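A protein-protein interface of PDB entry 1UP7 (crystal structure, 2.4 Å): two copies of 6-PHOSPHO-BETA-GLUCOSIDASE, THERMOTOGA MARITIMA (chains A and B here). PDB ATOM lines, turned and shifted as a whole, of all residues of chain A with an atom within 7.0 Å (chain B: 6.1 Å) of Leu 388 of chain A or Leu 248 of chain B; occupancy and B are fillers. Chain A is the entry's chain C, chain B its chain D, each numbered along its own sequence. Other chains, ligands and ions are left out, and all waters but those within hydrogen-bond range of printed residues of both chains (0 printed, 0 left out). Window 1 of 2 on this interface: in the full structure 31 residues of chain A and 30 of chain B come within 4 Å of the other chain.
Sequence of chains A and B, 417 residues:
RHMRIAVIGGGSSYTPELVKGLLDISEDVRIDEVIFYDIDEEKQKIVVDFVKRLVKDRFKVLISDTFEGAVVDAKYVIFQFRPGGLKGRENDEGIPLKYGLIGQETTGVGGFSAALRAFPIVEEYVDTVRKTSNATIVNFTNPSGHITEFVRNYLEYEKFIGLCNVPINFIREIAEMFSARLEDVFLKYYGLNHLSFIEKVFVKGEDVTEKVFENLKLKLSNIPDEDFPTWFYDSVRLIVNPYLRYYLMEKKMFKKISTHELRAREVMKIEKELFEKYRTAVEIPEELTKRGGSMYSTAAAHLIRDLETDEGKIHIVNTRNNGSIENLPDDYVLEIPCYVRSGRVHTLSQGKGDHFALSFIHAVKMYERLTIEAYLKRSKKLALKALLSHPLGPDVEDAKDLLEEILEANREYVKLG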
ATOM      1  N   TYR A 367     -32.876  20.619 -35.745  1.00  0.00           N
ATOM      2  CA  TYR A 367     -32.527  21.915 -36.291  1.00  0.00           C
ATOM      3  C   TYR A 367     -33.665  22.431 -37.233  1.00  0.00           C
ATOM      4  O   TYR A 367     -34.072  23.602 -37.129  1.00  0.00           O
ATOM      5  CB  TYR A 367     -31.139  21.936 -36.969  1.00  0.00           C
ATOM      6  CG  TYR A 367     -31.138  22.888 -38.158  1.00  0.00           C
ATOM      7  CD1 TYR A 367     -30.839  24.260 -37.980  1.00  0.00           C
ATOM      8  CD2 TYR A 367     -31.498  22.441 -39.443  1.00  0.00           C
ATOM      9  CE1 TYR A 367     -30.877  25.134 -39.030  1.00  0.00           C
ATOM     10  CE2 TYR A 367     -31.551  23.315 -40.506  1.00  0.00           C
ATOM     11  CZ  TYR A 367     -31.238  24.674 -40.301  1.00  0.00           C
ATOM     12  OH  TYR A 367     -31.288  25.576 -41.353  1.00  0.00           O
ATOM     13  N   LEU A 370     -36.705  23.669 -35.145  1.00  0.00           N
ATOM     14  CA  LEU A 370     -36.318  24.873 -34.412  1.00  0.00           C
ATOM     15  C   LEU A 370     -36.296  26.070 -35.347  1.00  0.00           C
ATOM     16  O   LEU A 370     -36.734  27.169 -34.982  1.00  0.00           O
ATOM     17  CB  LEU A 370     -34.959  24.701 -33.716  1.00  0.00           C
ATOM     18  CG  LEU A 370     -34.934  23.780 -32.471  1.00  0.00           C
ATOM     19  CD1 LEU A 370     -33.519  23.370 -32.068  1.00  0.00           C
ATOM     20  CD2 LEU A 370     -35.686  24.410 -31.300  1.00  0.00           C
ATOM     21  N   LEU A 382     -35.349  32.634 -30.672  1.00  0.00           N
ATOM     22  CA  LEU A 382     -35.500  31.264 -31.151  1.00  0.00           C
ATOM     23  C   LEU A 382     -34.654  30.985 -32.388  1.00  0.00           C
ATOM     24  O   LEU A 382     -34.253  29.847 -32.612  1.00  0.00           O
ATOM     25  CB  LEU A 382     -36.980  30.916 -31.368  1.00  0.00           C
ATOM     26  CG  LEU A 382     -37.842  30.941 -30.095  1.00  0.00           C
ATOM     27  CD1 LEU A 382     -39.288  30.506 -30.397  1.00  0.00           C
ATOM     28  CD2 LEU A 382     -37.224  30.079 -28.926  1.00  0.00           C
ATOM     29  N   ALA A 383     -34.350  32.014 -33.178  1.00  0.00           N
ATOM     30  CA  ALA A 383     -33.490  31.823 -34.331  1.00  0.00           C
ATOM     31  C   ALA A 383     -32.051  31.480 -33.881  1.00  0.00           C
ATOM     32  O   ALA A 383     -31.406  30.595 -34.449  1.00  0.00           O
ATOM     33  CB  ALA A 383     -33.527  33.029 -35.236  1.00  0.00           C
ATOM     34  N   LEU A 384     -31.582  32.155 -32.831  1.00  0.00           N
ATOM     35  CA  LEU A 384     -30.291  31.848 -32.204  1.00  0.00           C
ATOM     36  C   LEU A 384     -30.240  30.403 -31.742  1.00  0.00           C
ATOM     37  O   LEU A 384     -29.234  29.697 -31.911  1.00  0.00           O
ATOM     38  CB  LEU A 384     -30.069  32.735 -30.981  1.00  0.00           C
ATOM     39  CG  LEU A 384     -28.999  33.820 -30.894  1.00  0.00           C
ATOM     40  CD1 LEU A 384     -28.347  34.244 -32.233  1.00  0.00           C
ATOM     41  CD2 LEU A 384     -29.588  35.066 -30.147  1.00  0.00           C
ATOM     42  N   LYS A 385     -31.334  29.973 -31.133  1.00  0.00           N
ATOM     43  CA  LYS A 385     -31.460  28.622 -30.659  1.00  0.00           C
ATOM     44  C   LYS A 385     -31.391  27.627 -31.828  1.00  0.00           C
ATOM     45  O   LYS A 385     -30.684  26.580 -31.736  1.00  0.00           O
ATOM     46  CB  LYS A 385     -32.741  28.502 -29.835  1.00  0.00           C
ATOM     47  CG  LYS A 385     -33.112  27.145 -29.369  1.00  0.00           C
ATOM     48  CD  LYS A 385     -34.350  27.259 -28.479  1.00  0.00           C
ATOM     49  CE  LYS A 385     -34.780  25.924 -27.952  1.00  0.00           C
ATOM     50  NZ  LYS A 385     -35.651  26.059 -26.782  1.00  0.00           N
ATOM     51  N   ALA A 386     -32.100  27.942 -32.914  1.00  0.00           N
ATOM     52  CA  ALA A 386     -32.047  27.083 -34.109  1.00  0.00           C
ATOM     53  C   ALA A 386     -30.615  26.995 -34.662  1.00  0.00           C
ATOM     54  O   ALA A 386     -30.112  25.900 -34.944  1.00  0.00           O
ATOM     55  CB  ALA A 386     -33.012  27.554 -35.181  1.00  0.00           C
ATOM     56  N   LEU A 387     -29.960  28.146 -34.750  1.00  0.00           N
ATOM     57  CA  LEU A 387     -28.633  28.247 -35.314  1.00  0.00           C
ATOM     58  C   LEU A 387     -27.606  27.457 -34.522  1.00  0.00           C
ATOM     59  O   LEU A 387     -26.725  26.794 -35.096  1.00  0.00           O
ATOM     60  CB  LEU A 387     -28.239  29.730 -35.391  1.00  0.00           C
ATOM     61  CG  LEU A 387     -27.458  30.351 -36.548  1.00  0.00           C
ATOM     62  CD1 LEU A 387     -27.663  29.774 -37.951  1.00  0.00           C
ATOM     63  CD2 LEU A 387     -27.645  31.855 -36.505  1.00  0.00           C
ATOM     64  N   LEU A 388     -27.709  27.501 -33.195  1.00  0.00           N
ATOM     65  CA  LEU A 388     -26.811  26.745 -32.347  1.00  0.00           C
ATOM     66  C   LEU A 388     -27.002  25.260 -32.429  1.00  0.00           C
ATOM     67  O   LEU A 388     -26.100  24.502 -32.039  1.00  0.00           O
ATOM     68  CB  LEU A 388     -27.009  27.099 -30.884  1.00  0.00           C
ATOM     69  CG  LEU A 388     -26.603  28.490 -30.475  1.00  0.00           C
ATOM     70  CD1 LEU A 388     -27.228  28.721 -29.114  1.00  0.00           C
ATOM     71  CD2 LEU A 388     -25.052  28.641 -30.479  1.00  0.00           C
ATOM     72  N   SER A 389     -28.182  24.826 -32.853  1.00  0.00           N
ATOM     73  CA  SER A 389     -28.475  23.399 -32.861  1.00  0.00           C
ATOM     74  C   SER A 389     -27.962  22.704 -34.128  1.00  0.00           C
ATOM     75  O   SER A 389     -27.921  21.491 -34.186  1.00  0.00           O
ATOM     76  CB  SER A 389     -29.970  23.164 -32.724  1.00  0.00           C
ATOM     77  OG  SER A 389     -30.629  23.503 -33.934  1.00  0.00           O
ATOM     78  N   HIS A 390     -27.618  23.460 -35.159  1.00  0.00           N
ATOM     79  CA  HIS A 390     -27.118  22.815 -36.366  1.00  0.00           C
ATOM     80  C   HIS A 390     -25.707  22.263 -36.123  1.00  0.00           C
ATOM     81  O   HIS A 390     -24.854  22.993 -35.621  1.00  0.00           O
ATOM     82  CB  HIS A 390     -27.095  23.767 -37.567  1.00  0.00           C
ATOM     83  CG  HIS A 390     -27.027  23.054 -38.890  1.00  0.00           C
ATOM     84  ND1 HIS A 390     -25.878  22.428 -39.348  1.00  0.00           N
ATOM     85  CD2 HIS A 390     -27.977  22.850 -39.844  1.00  0.00           C
ATOM     86  CE1 HIS A 390     -26.125  21.877 -40.525  1.00  0.00           C
ATOM     87  NE2 HIS A 390     -27.390  22.125 -40.853  1.00  0.00           N
ATOM     88  N   PRO A 391     -25.453  21.011 -36.519  1.00  0.00           N
ATOM     89  CA  PRO A 391     -24.104  20.450 -36.427  1.00  0.00           C
ATOM     90  C   PRO A 391     -23.045  21.350 -37.058  1.00  0.00           C
ATOM     91  O   PRO A 391     -21.924  21.303 -36.623  1.00  0.00           O
ATOM     92  CB  PRO A 391     -24.199  19.132 -37.207  1.00  0.00           C
ATOM     93  CG  PRO A 391     -25.603  18.730 -37.075  1.00  0.00           C
ATOM     94  CD  PRO A 391     -26.416  20.034 -37.061  1.00  0.00           C
ATOM     95  N   GLY A 393     -23.427  24.744 -37.347  1.00  0.00           N
ATOM     96  CA  GLY A 393     -23.644  26.095 -36.872  1.00  0.00           C
ATOM     97  C   GLY A 393     -22.558  26.674 -35.982  1.00  0.00           C
ATOM     98  O   GLY A 393     -21.583  26.029 -35.666  1.00  0.00           O
ATOM     99  N   PRO A 394     -22.744  27.915 -35.560  1.00  0.00           N
ATOM    100  CA  PRO A 394     -21.736  28.636 -34.786  1.00  0.00           C
ATOM    101  C   PRO A 394     -21.602  28.153 -33.348  1.00  0.00           C
ATOM    102  O   PRO A 394     -22.527  27.588 -32.780  1.00  0.00           O
ATOM    103  CB  PRO A 394     -22.279  30.065 -34.789  1.00  0.00           C
ATOM    104  CG  PRO A 394     -23.774  29.876 -34.916  1.00  0.00           C
ATOM    105  CD  PRO A 394     -23.951  28.724 -35.809  1.00  0.00           C
ATOM    106  N   ASP A 395     -20.423  28.371 -32.786  1.00  0.00           N
ATOM    107  CA  ASP A 395     -20.199  28.311 -31.352  1.00  0.00           C
ATOM    108  C   ASP A 395     -20.984  29.487 -30.759  1.00  0.00           C
ATOM    109  O   ASP A 395     -21.227  30.489 -31.437  1.00  0.00           O
ATOM    110  CB  ASP A 395     -18.720  28.569 -31.026  1.00  0.00           C
ATOM    111  CG  ASP A 395     -17.835  27.324 -31.146  1.00  0.00           C
ATOM    112  OD1 ASP A 395     -18.278  26.278 -31.647  1.00  0.00           O
ATOM    113  OD2 ASP A 395     -16.647  27.316 -30.746  1.00  0.00           O
ATOM    114  N   VAL A 396     -21.311  29.377 -29.485  1.00  0.00           N
ATOM    115  CA  VAL A 396     -21.959  30.422 -28.722  1.00  0.00           C
ATOM    116  C   VAL A 396     -21.320  31.790 -28.930  1.00  0.00           C
ATOM    117  O   VAL A 396     -22.024  32.766 -29.115  1.00  0.00           O
ATOM    118  CB  VAL A 396     -21.952  30.043 -27.225  1.00  0.00           C
ATOM    119  CG1 VAL A 396     -22.288  31.235 -26.356  1.00  0.00           C
ATOM    120  CG2 VAL A 396     -22.921  28.898 -26.975  1.00  0.00           C
ATOM    121  N   GLU A 397     -19.988  31.860 -28.921  1.00  0.00           N
ATOM    122  CA  GLU A 397     -19.273  33.125 -29.090  1.00  0.00           C
ATOM    123  C   GLU A 397     -19.515  33.804 -30.447  1.00  0.00           C
ATOM    124  O   GLU A 397     -19.345  35.005 -30.567  1.00  0.00           O
ATOM    125  CB  GLU A 397     -17.770  32.947 -28.839  1.00  0.00           C
ATOM    126  CG  GLU A 397     -17.021  32.158 -29.914  1.00  0.00           C
ATOM    127  CD  GLU A 397     -15.500  32.099 -29.675  1.00  0.00           C
ATOM    128  OE1 GLU A 397     -14.791  33.077 -30.006  1.00  0.00           O
ATOM    129  OE2 GLU A 397     -15.004  31.073 -29.170  1.00  0.00           O
ATOM    130  N   ASP A 398     -19.918  33.053 -31.471  1.00  0.00           N
ATOM    131  CA  ASP A 398     -20.120  33.678 -32.786  1.00  0.00           C
ATOM    132  C   ASP A 398     -21.578  33.885 -33.136  1.00  0.00           C
ATOM    133  O   ASP A 398     -21.849  34.576 -34.093  1.00  0.00           O
ATOM    134  CB  ASP A 398     -19.485  32.865 -33.913  1.00  0.00           C
ATOM    135  CG  ASP A 398     -18.004  32.725 -33.746  1.00  0.00           C
ATOM    136  OD1 ASP A 398     -17.357  33.766 -33.567  1.00  0.00           O
ATOM    137  OD2 ASP A 398     -17.409  31.621 -33.741  1.00  0.00           O
ATOM    138  N   ALA A 399     -22.497  33.286 -32.376  1.00  0.00           N
ATOM    139  CA  ALA A 399     -23.860  33.101 -32.850  1.00  0.00           C
ATOM    140  C   ALA A 399     -24.626  34.427 -33.016  1.00  0.00           C
ATOM    141  O   ALA A 399     -25.323  34.639 -34.025  1.00  0.00           O
ATOM    142  CB  ALA A 399     -24.601  32.158 -31.942  1.00  0.00           C
ATOM    143  N   LYS A 400     -24.470  35.329 -32.044  1.00  0.00           N
ATOM    144  CA  LYS A 400     -25.134  36.636 -32.124  1.00  0.00           C
ATOM    145  C   LYS A 400     -24.712  37.478 -33.302  1.00  0.00           C
ATOM    146  O   LYS A 400     -25.559  38.030 -33.999  1.00  0.00           O
ATOM    147  CB  LYS A 400     -24.950  37.460 -30.857  1.00  0.00           C
ATOM    148  CG  LYS A 400     -25.963  37.144 -29.803  1.00  0.00           C
ATOM    149  CD  LYS A 400     -26.129  38.282 -28.822  1.00  0.00           C
ATOM    150  CE  LYS A 400     -27.594  38.722 -28.788  1.00  0.00           C
ATOM    151  NZ  LYS A 400     -27.683  40.205 -28.528  1.00  0.00           N
ATOM    152  N   PHE B 228     -21.902  30.383 -20.056  1.00  0.00           N
ATOM    153  CA  PHE B 228     -22.876  30.804 -21.028  1.00  0.00           C
ATOM    154  C   PHE B 228     -23.282  32.232 -20.738  1.00  0.00           C
ATOM    155  O   PHE B 228     -23.486  32.608 -19.585  1.00  0.00           O
ATOM    156  CB  PHE B 228     -24.055  29.835 -21.030  1.00  0.00           C
ATOM    157  CG  PHE B 228     -23.692  28.469 -21.531  1.00  0.00           C
ATOM    158  CD1 PHE B 228     -23.575  28.219 -22.895  1.00  0.00           C
ATOM    159  CD2 PHE B 228     -23.424  27.438 -20.643  1.00  0.00           C
ATOM    160  CE1 PHE B 228     -23.237  26.952 -23.355  1.00  0.00           C
ATOM    161  CE2 PHE B 228     -23.100  26.173 -21.109  1.00  0.00           C
ATOM    162  CZ  PHE B 228     -23.023  25.932 -22.471  1.00  0.00           C
ATOM    163  N   TRP B 231     -27.756  36.135 -22.805  1.00  0.00           N
ATOM    164  CA  TRP B 231     -28.634  35.889 -23.963  1.00  0.00           C
ATOM    165  C   TRP B 231     -28.880  34.388 -24.206  1.00  0.00           C
ATOM    166  O   TRP B 231     -29.944  34.013 -24.709  1.00  0.00           O
ATOM    167  CB  TRP B 231     -28.158  36.610 -25.238  1.00  0.00           C
ATOM    168  CG  TRP B 231     -26.860  36.093 -25.825  1.00  0.00           C
ATOM    169  CD1 TRP B 231     -25.627  36.686 -25.732  1.00  0.00           C
ATOM    170  CD2 TRP B 231     -26.669  34.885 -26.596  1.00  0.00           C
ATOM    171  NE1 TRP B 231     -24.686  35.913 -26.374  1.00  0.00           N
ATOM    172  CE2 TRP B 231     -25.292  34.809 -26.920  1.00  0.00           C
ATOM    173  CE3 TRP B 231     -27.522  33.862 -27.046  1.00  0.00           C
ATOM    174  CZ2 TRP B 231     -24.749  33.768 -27.685  1.00  0.00           C
ATOM    175  CZ3 TRP B 231     -26.973  32.794 -27.788  1.00  0.00           C
ATOM    176  CH2 TRP B 231     -25.596  32.771 -28.108  1.00  0.00           C
ATOM    177  N   PHE B 232     -27.934  33.540 -23.803  1.00  0.00           N
ATOM    178  CA  PHE B 232     -28.049  32.098 -24.052  1.00  0.00           C
ATOM    179  C   PHE B 232     -29.222  31.507 -23.278  1.00  0.00           C
ATOM    180  O   PHE B 232     -30.011  30.732 -23.825  1.00  0.00           O
ATOM    181  CB  PHE B 232     -26.714  31.345 -23.800  1.00  0.00           C
ATOM    182  CG  PHE B 232     -26.826  29.849 -23.902  1.00  0.00           C
ATOM    183  CD1 PHE B 232     -27.220  29.096 -22.807  1.00  0.00           C
ATOM    184  CD2 PHE B 232     -26.567  29.192 -25.110  1.00  0.00           C
ATOM    185  CE1 PHE B 232     -27.357  27.718 -22.910  1.00  0.00           C
ATOM    186  CE2 PHE B 232     -26.679  27.834 -25.222  1.00  0.00           C
ATOM    187  CZ  PHE B 232     -27.070  27.078 -24.122  1.00  0.00           C
ATOM    188  N   SER B 235     -32.506  32.633 -24.739  1.00  0.00           N
ATOM    189  CA  SER B 235     -32.789  32.091 -26.060  1.00  0.00           C
ATOM    190  C   SER B 235     -33.181  30.648 -26.001  1.00  0.00           C
ATOM    191  O   SER B 235     -34.201  30.265 -26.549  1.00  0.00           O
ATOM    192  CB  SER B 235     -31.569  32.230 -26.967  1.00  0.00           C
ATOM    193  OG  SER B 235     -31.471  33.593 -27.385  1.00  0.00           O
ATOM    194  N   VAL B 236     -32.363  29.855 -25.317  1.00  0.00           N
ATOM    195  CA  VAL B 236     -32.475  28.410 -25.323  1.00  0.00           C
ATOM    196  C   VAL B 236     -33.511  27.987 -24.283  1.00  0.00           C
ATOM    197  O   VAL B 236     -34.236  27.015 -24.484  1.00  0.00           O
ATOM    198  CB  VAL B 236     -31.093  27.774 -25.069  1.00  0.00           C
ATOM    199  CG1 VAL B 236     -31.172  26.248 -24.925  1.00  0.00           C
ATOM    200  CG2 VAL B 236     -30.135  28.177 -26.180  1.00  0.00           C
ATOM    201  N   VAL B 240     -28.438  24.081 -18.527  1.00  0.00           N
ATOM    202  CA  VAL B 240     -27.678  23.142 -19.296  1.00  0.00           C
ATOM    203  C   VAL B 240     -26.529  22.594 -18.453  1.00  0.00           C
ATOM    204  O   VAL B 240     -25.916  23.321 -17.679  1.00  0.00           O
ATOM    205  CB  VAL B 240     -27.193  23.899 -20.545  1.00  0.00           C
ATOM    206  CG1 VAL B 240     -25.733  24.079 -20.544  1.00  0.00           C
ATOM    207  CG2 VAL B 240     -27.765  23.287 -21.827  1.00  0.00           C
ATOM    208  N   LEU B 244     -21.945  20.560 -21.562  1.00  0.00           N
ATOM    209  CA  LEU B 244     -22.372  21.065 -22.862  1.00  0.00           C
ATOM    210  C   LEU B 244     -21.451  22.157 -23.402  1.00  0.00           C
ATOM    211  O   LEU B 244     -21.477  22.419 -24.584  1.00  0.00           O
ATOM    212  CB  LEU B 244     -23.817  21.602 -22.842  1.00  0.00           C
ATOM    213  CG  LEU B 244     -24.935  20.669 -23.341  1.00  0.00           C
ATOM    214  CD1 LEU B 244     -24.728  20.256 -24.803  1.00  0.00           C
ATOM    215  CD2 LEU B 244     -25.097  19.415 -22.412  1.00  0.00           C
ATOM    216  N   ARG B 245     -20.664  22.803 -22.555  1.00  0.00           N
ATOM    217  CA  ARG B 245     -19.653  23.737 -23.049  1.00  0.00           C
ATOM    218  C   ARG B 245     -18.705  23.123 -24.076  1.00  0.00           C
ATOM    219  O   ARG B 245     -18.282  23.812 -25.009  1.00  0.00           O
ATOM    220  CB  ARG B 245     -18.801  24.304 -21.920  1.00  0.00           C
ATOM    221  CG  ARG B 245     -19.510  25.333 -21.070  1.00  0.00           C
ATOM    222  CD  ARG B 245     -18.692  25.745 -19.854  1.00  0.00           C
ATOM    223  NE  ARG B 245     -18.219  24.540 -19.156  1.00  0.00           N
ATOM    224  CZ  ARG B 245     -17.148  24.483 -18.357  1.00  0.00           C
ATOM    225  NH1 ARG B 245     -16.422  25.578 -18.134  1.00  0.00           N
ATOM    226  NH2 ARG B 245     -16.812  23.326 -17.786  1.00  0.00           N
ATOM    227  N   TYR B 246     -18.376  21.845 -23.922  1.00  0.00           N
ATOM    228  CA  TYR B 246     -17.472  21.203 -24.867  1.00  0.00           C
ATOM    229  C   TYR B 246     -18.126  21.101 -26.231  1.00  0.00           C
ATOM    230  O   TYR B 246     -17.440  21.028 -27.229  1.00  0.00           O
ATOM    231  CB  TYR B 246     -17.055  19.827 -24.362  1.00  0.00           C
ATOM    232  CG  TYR B 246     -16.286  19.911 -23.060  1.00  0.00           C
ATOM    233  CD1 TYR B 246     -14.998  20.413 -23.046  1.00  0.00           C
ATOM    234  CD2 TYR B 246     -16.862  19.508 -21.842  1.00  0.00           C
ATOM    235  CE1 TYR B 246     -14.280  20.507 -21.884  1.00  0.00           C
ATOM    236  CE2 TYR B 246     -16.135  19.602 -20.653  1.00  0.00           C
ATOM    237  CZ  TYR B 246     -14.843  20.100 -20.701  1.00  0.00           C
ATOM    238  OH  TYR B 246     -14.082  20.227 -19.578  1.00  0.00           O
ATOM    239  N   TYR B 247     -19.457  21.092 -26.265  1.00  0.00           N
ATOM    240  CA  TYR B 247     -20.190  20.959 -27.522  1.00  0.00           C
ATOM    241  C   TYR B 247     -20.411  22.354 -28.113  1.00  0.00           C
ATOM    242  O   TYR B 247     -20.009  22.631 -29.251  1.00  0.00           O
ATOM    243  CB  TYR B 247     -21.534  20.240 -27.308  1.00  0.00           C
ATOM    244  CG  TYR B 247     -21.428  18.751 -27.025  1.00  0.00           C
ATOM    245  CD1 TYR B 247     -21.222  18.269 -25.716  1.00  0.00           C
ATOM    246  CD2 TYR B 247     -21.524  17.816 -28.065  1.00  0.00           C
ATOM    247  CE1 TYR B 247     -21.132  16.901 -25.449  1.00  0.00           C
ATOM    248  CE2 TYR B 247     -21.431  16.442 -27.815  1.00  0.00           C
ATOM    249  CZ  TYR B 247     -21.236  15.997 -26.503  1.00  0.00           C
ATOM    250  OH  TYR B 247     -21.146  14.650 -26.262  1.00  0.00           O
ATOM    251  N   LEU B 248     -20.975  23.248 -27.304  1.00  0.00           N
ATOM    252  CA  LEU B 248     -21.467  24.530 -27.757  1.00  0.00           C
ATOM    253  C   LEU B 248     -20.408  25.632 -27.706  1.00  0.00           C
ATOM    254  O   LEU B 248     -20.540  26.668 -28.360  1.00  0.00           O
ATOM    255  CB  LEU B 248     -22.685  24.910 -26.927  1.00  0.00           C
ATOM    256  CG  LEU B 248     -24.002  24.146 -27.198  1.00  0.00           C
ATOM    257  CD1 LEU B 248     -24.957  24.432 -26.087  1.00  0.00           C
ATOM    258  CD2 LEU B 248     -24.637  24.554 -28.551  1.00  0.00           C
ATOM    259  N   MET B 249     -19.341  25.395 -26.949  1.00  0.00           N
ATOM    260  CA  MET B 249     -18.218  26.319 -26.908  1.00  0.00           C
ATOM    261  C   MET B 249     -16.910  25.560 -27.202  1.00  0.00           C
ATOM    262  O   MET B 249     -15.893  25.781 -26.520  1.00  0.00           O
ATOM    263  CB  MET B 249     -18.116  26.959 -25.518  1.00  0.00           C
ATOM    264  CG  MET B 249     -19.374  27.671 -24.958  1.00  0.00           C
ATOM    265  SD  MET B 249     -18.968  28.571 -23.365  1.00  0.00           S
ATOM    266  CE  MET B 249     -20.375  29.427 -23.169  1.00  0.00           C
ATOM    267  N   GLU B 250     -16.938  24.689 -28.219  1.00  0.00           N
ATOM    268  CA  GLU B 250     -15.812  23.810 -28.550  1.00  0.00           C
ATOM    269  C   GLU B 250     -14.512  24.574 -28.677  1.00  0.00           C
ATOM    270  O   GLU B 250     -13.527  24.213 -28.033  1.00  0.00           O
ATOM    271  CB  GLU B 250     -16.077  22.994 -29.835  1.00  0.00           C
ATOM    272  CG  GLU B 250     -15.045  21.897 -30.076  1.00  0.00           C
ATOM    273  CD  GLU B 250     -15.298  21.111 -31.336  1.00  0.00           C
ATOM    274  OE1 GLU B 250     -16.418  21.239 -31.916  1.00  0.00           O
ATOM    275  OE2 GLU B 250     -14.366  20.360 -31.735  1.00  0.00           O
ATOM    276  N   PHE B 356     -34.075  21.282 -29.021  1.00  0.00           N
ATOM    277  CA  PHE B 356     -32.669  21.634 -28.853  1.00  0.00           C
ATOM    278  C   PHE B 356     -31.952  20.556 -28.060  1.00  0.00           C
ATOM    279  O   PHE B 356     -30.898  20.134 -28.464  1.00  0.00           O
ATOM    280  CB  PHE B 356     -32.536  23.017 -28.192  1.00  0.00           C
ATOM    281  CG  PHE B 356     -31.102  23.483 -27.967  1.00  0.00           C
ATOM    282  CD1 PHE B 356     -30.426  23.171 -26.782  1.00  0.00           C
ATOM    283  CD2 PHE B 356     -30.456  24.269 -28.913  1.00  0.00           C
ATOM    284  CE1 PHE B 356     -29.126  23.643 -26.555  1.00  0.00           C
ATOM    285  CE2 PHE B 356     -29.151  24.741 -28.700  1.00  0.00           C
ATOM    286  CZ  PHE B 356     -28.484  24.424 -27.508  1.00  0.00           C
ATOM    287  N   PHE B 360     -28.941  16.916 -29.311  1.00  0.00           N
ATOM    288  CA  PHE B 360     -27.781  16.294 -28.657  1.00  0.00           C
ATOM    289  C   PHE B 360     -27.998  14.888 -28.194  1.00  0.00           C
ATOM    290  O   PHE B 360     -27.145  14.061 -28.413  1.00  0.00           O
ATOM    291  CB  PHE B 360     -27.283  17.148 -27.491  1.00  0.00           C
ATOM    292  CG  PHE B 360     -26.733  18.452 -27.944  1.00  0.00           C
ATOM    293  CD1 PHE B 360     -25.468  18.517 -28.472  1.00  0.00           C
ATOM    294  CD2 PHE B 360     -27.505  19.597 -27.904  1.00  0.00           C
ATOM    295  CE1 PHE B 360     -24.953  19.692 -28.914  1.00  0.00           C
ATOM    296  CE2 PHE B 360     -26.987  20.794 -28.344  1.00  0.00           C
ATOM    297  CZ  PHE B 360     -25.703  20.835 -28.853  1.00  0.00           C
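The side-chain amino group (NZ) of Lys 385 of chain A is in hydrogen-bond range of the backbone carbonyl oxygen (O) of Val 236 of chain B.
The backbone NH (N) of Val 396 of chain A is in hydrogen-bond range of the backbone carbonyl oxygen (O) of Leu 248 of chain B.
O of Ala 386 of chain A is in hydrogen-bond range of OG of Ser 389 of chain A, at 2.7 Å.
O of Trp 231 of chain B sits at hydrogen-bond distance from OG of Ser 235 of chain B (3.1 Å).
Ser 235 of chain B touches Leu 382 of chain A.
Ser 235 of chain B touches Leu 384 of chain A (OG to CD2, 3.7 Å).
Ser 235 of chain B touches Lys 385 of chain A (O to CD, 3.6 Å).
O of Lys 385 of chain A touches CD2 of Phe 356 of chain B, at 3.7 Å.
O of Leu 388 of chain A touches CD2 of Leu 248 of chain B, at 3.8 Å.
CB of Leu 388 of chain A touches CE2 of Phe 356 of chain B, 3.9 Å away.
Ser 389 of chain A touches Phe 356 of chain B (CB to CD2, 3.998 Å).
CA of Asp 395 of chain A touches O of Leu 248 of chain B (3.4 Å).
Asp 395 of chain A touches Met 249 of chain B (OD2 to C, 3.96 Å).
Lys 400 of chain A touches Trp 231 of chain B (CD to CD1, 3.5 Å).
Printed residues of chain A within 4 Å of Ser 235 of chain B: Leu 382 (3.9 Å), Leu 384 (3.7 Å) and Lys 385 (3.6 Å).
Of the printed residues of chain A, Val 236 of chain B touches Lys 385.
Leu 248 of chain B touches just these residues of chain A: Leu 388 (3.8 Å), Asp 395 (3.4 Å) and Val 396 (3.0 Å).
The nearest residue of chain B that does not touch Leu 388 of chain A is Phe 232 of chain B (4.03 Å).
The nearest residue of chain A that does not touch Leu 248 of chain B is Pro 394 of chain A (4.9 Å).
Printed residues of chain B that touch a printed residue of chain A: Trp 231, Ser 235, Val 236, Leu 248, Met 249, Glu 250 and Phe 356.
Printed residues of chain A that touch a printed residue of chain B: Leu 370, Leu 382, Leu 384, Lys 385, Leu 388, Ser 389, Asp 395, Val 396 and Lys 400.
Along chain A the printed residues that touch a printed residue of chain B span positions 370 to 400.
No position is printed for both chains.
Of the 16 pairs that touch across the chains among the printed residues, none has its exchanged pair printed and touching as well.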
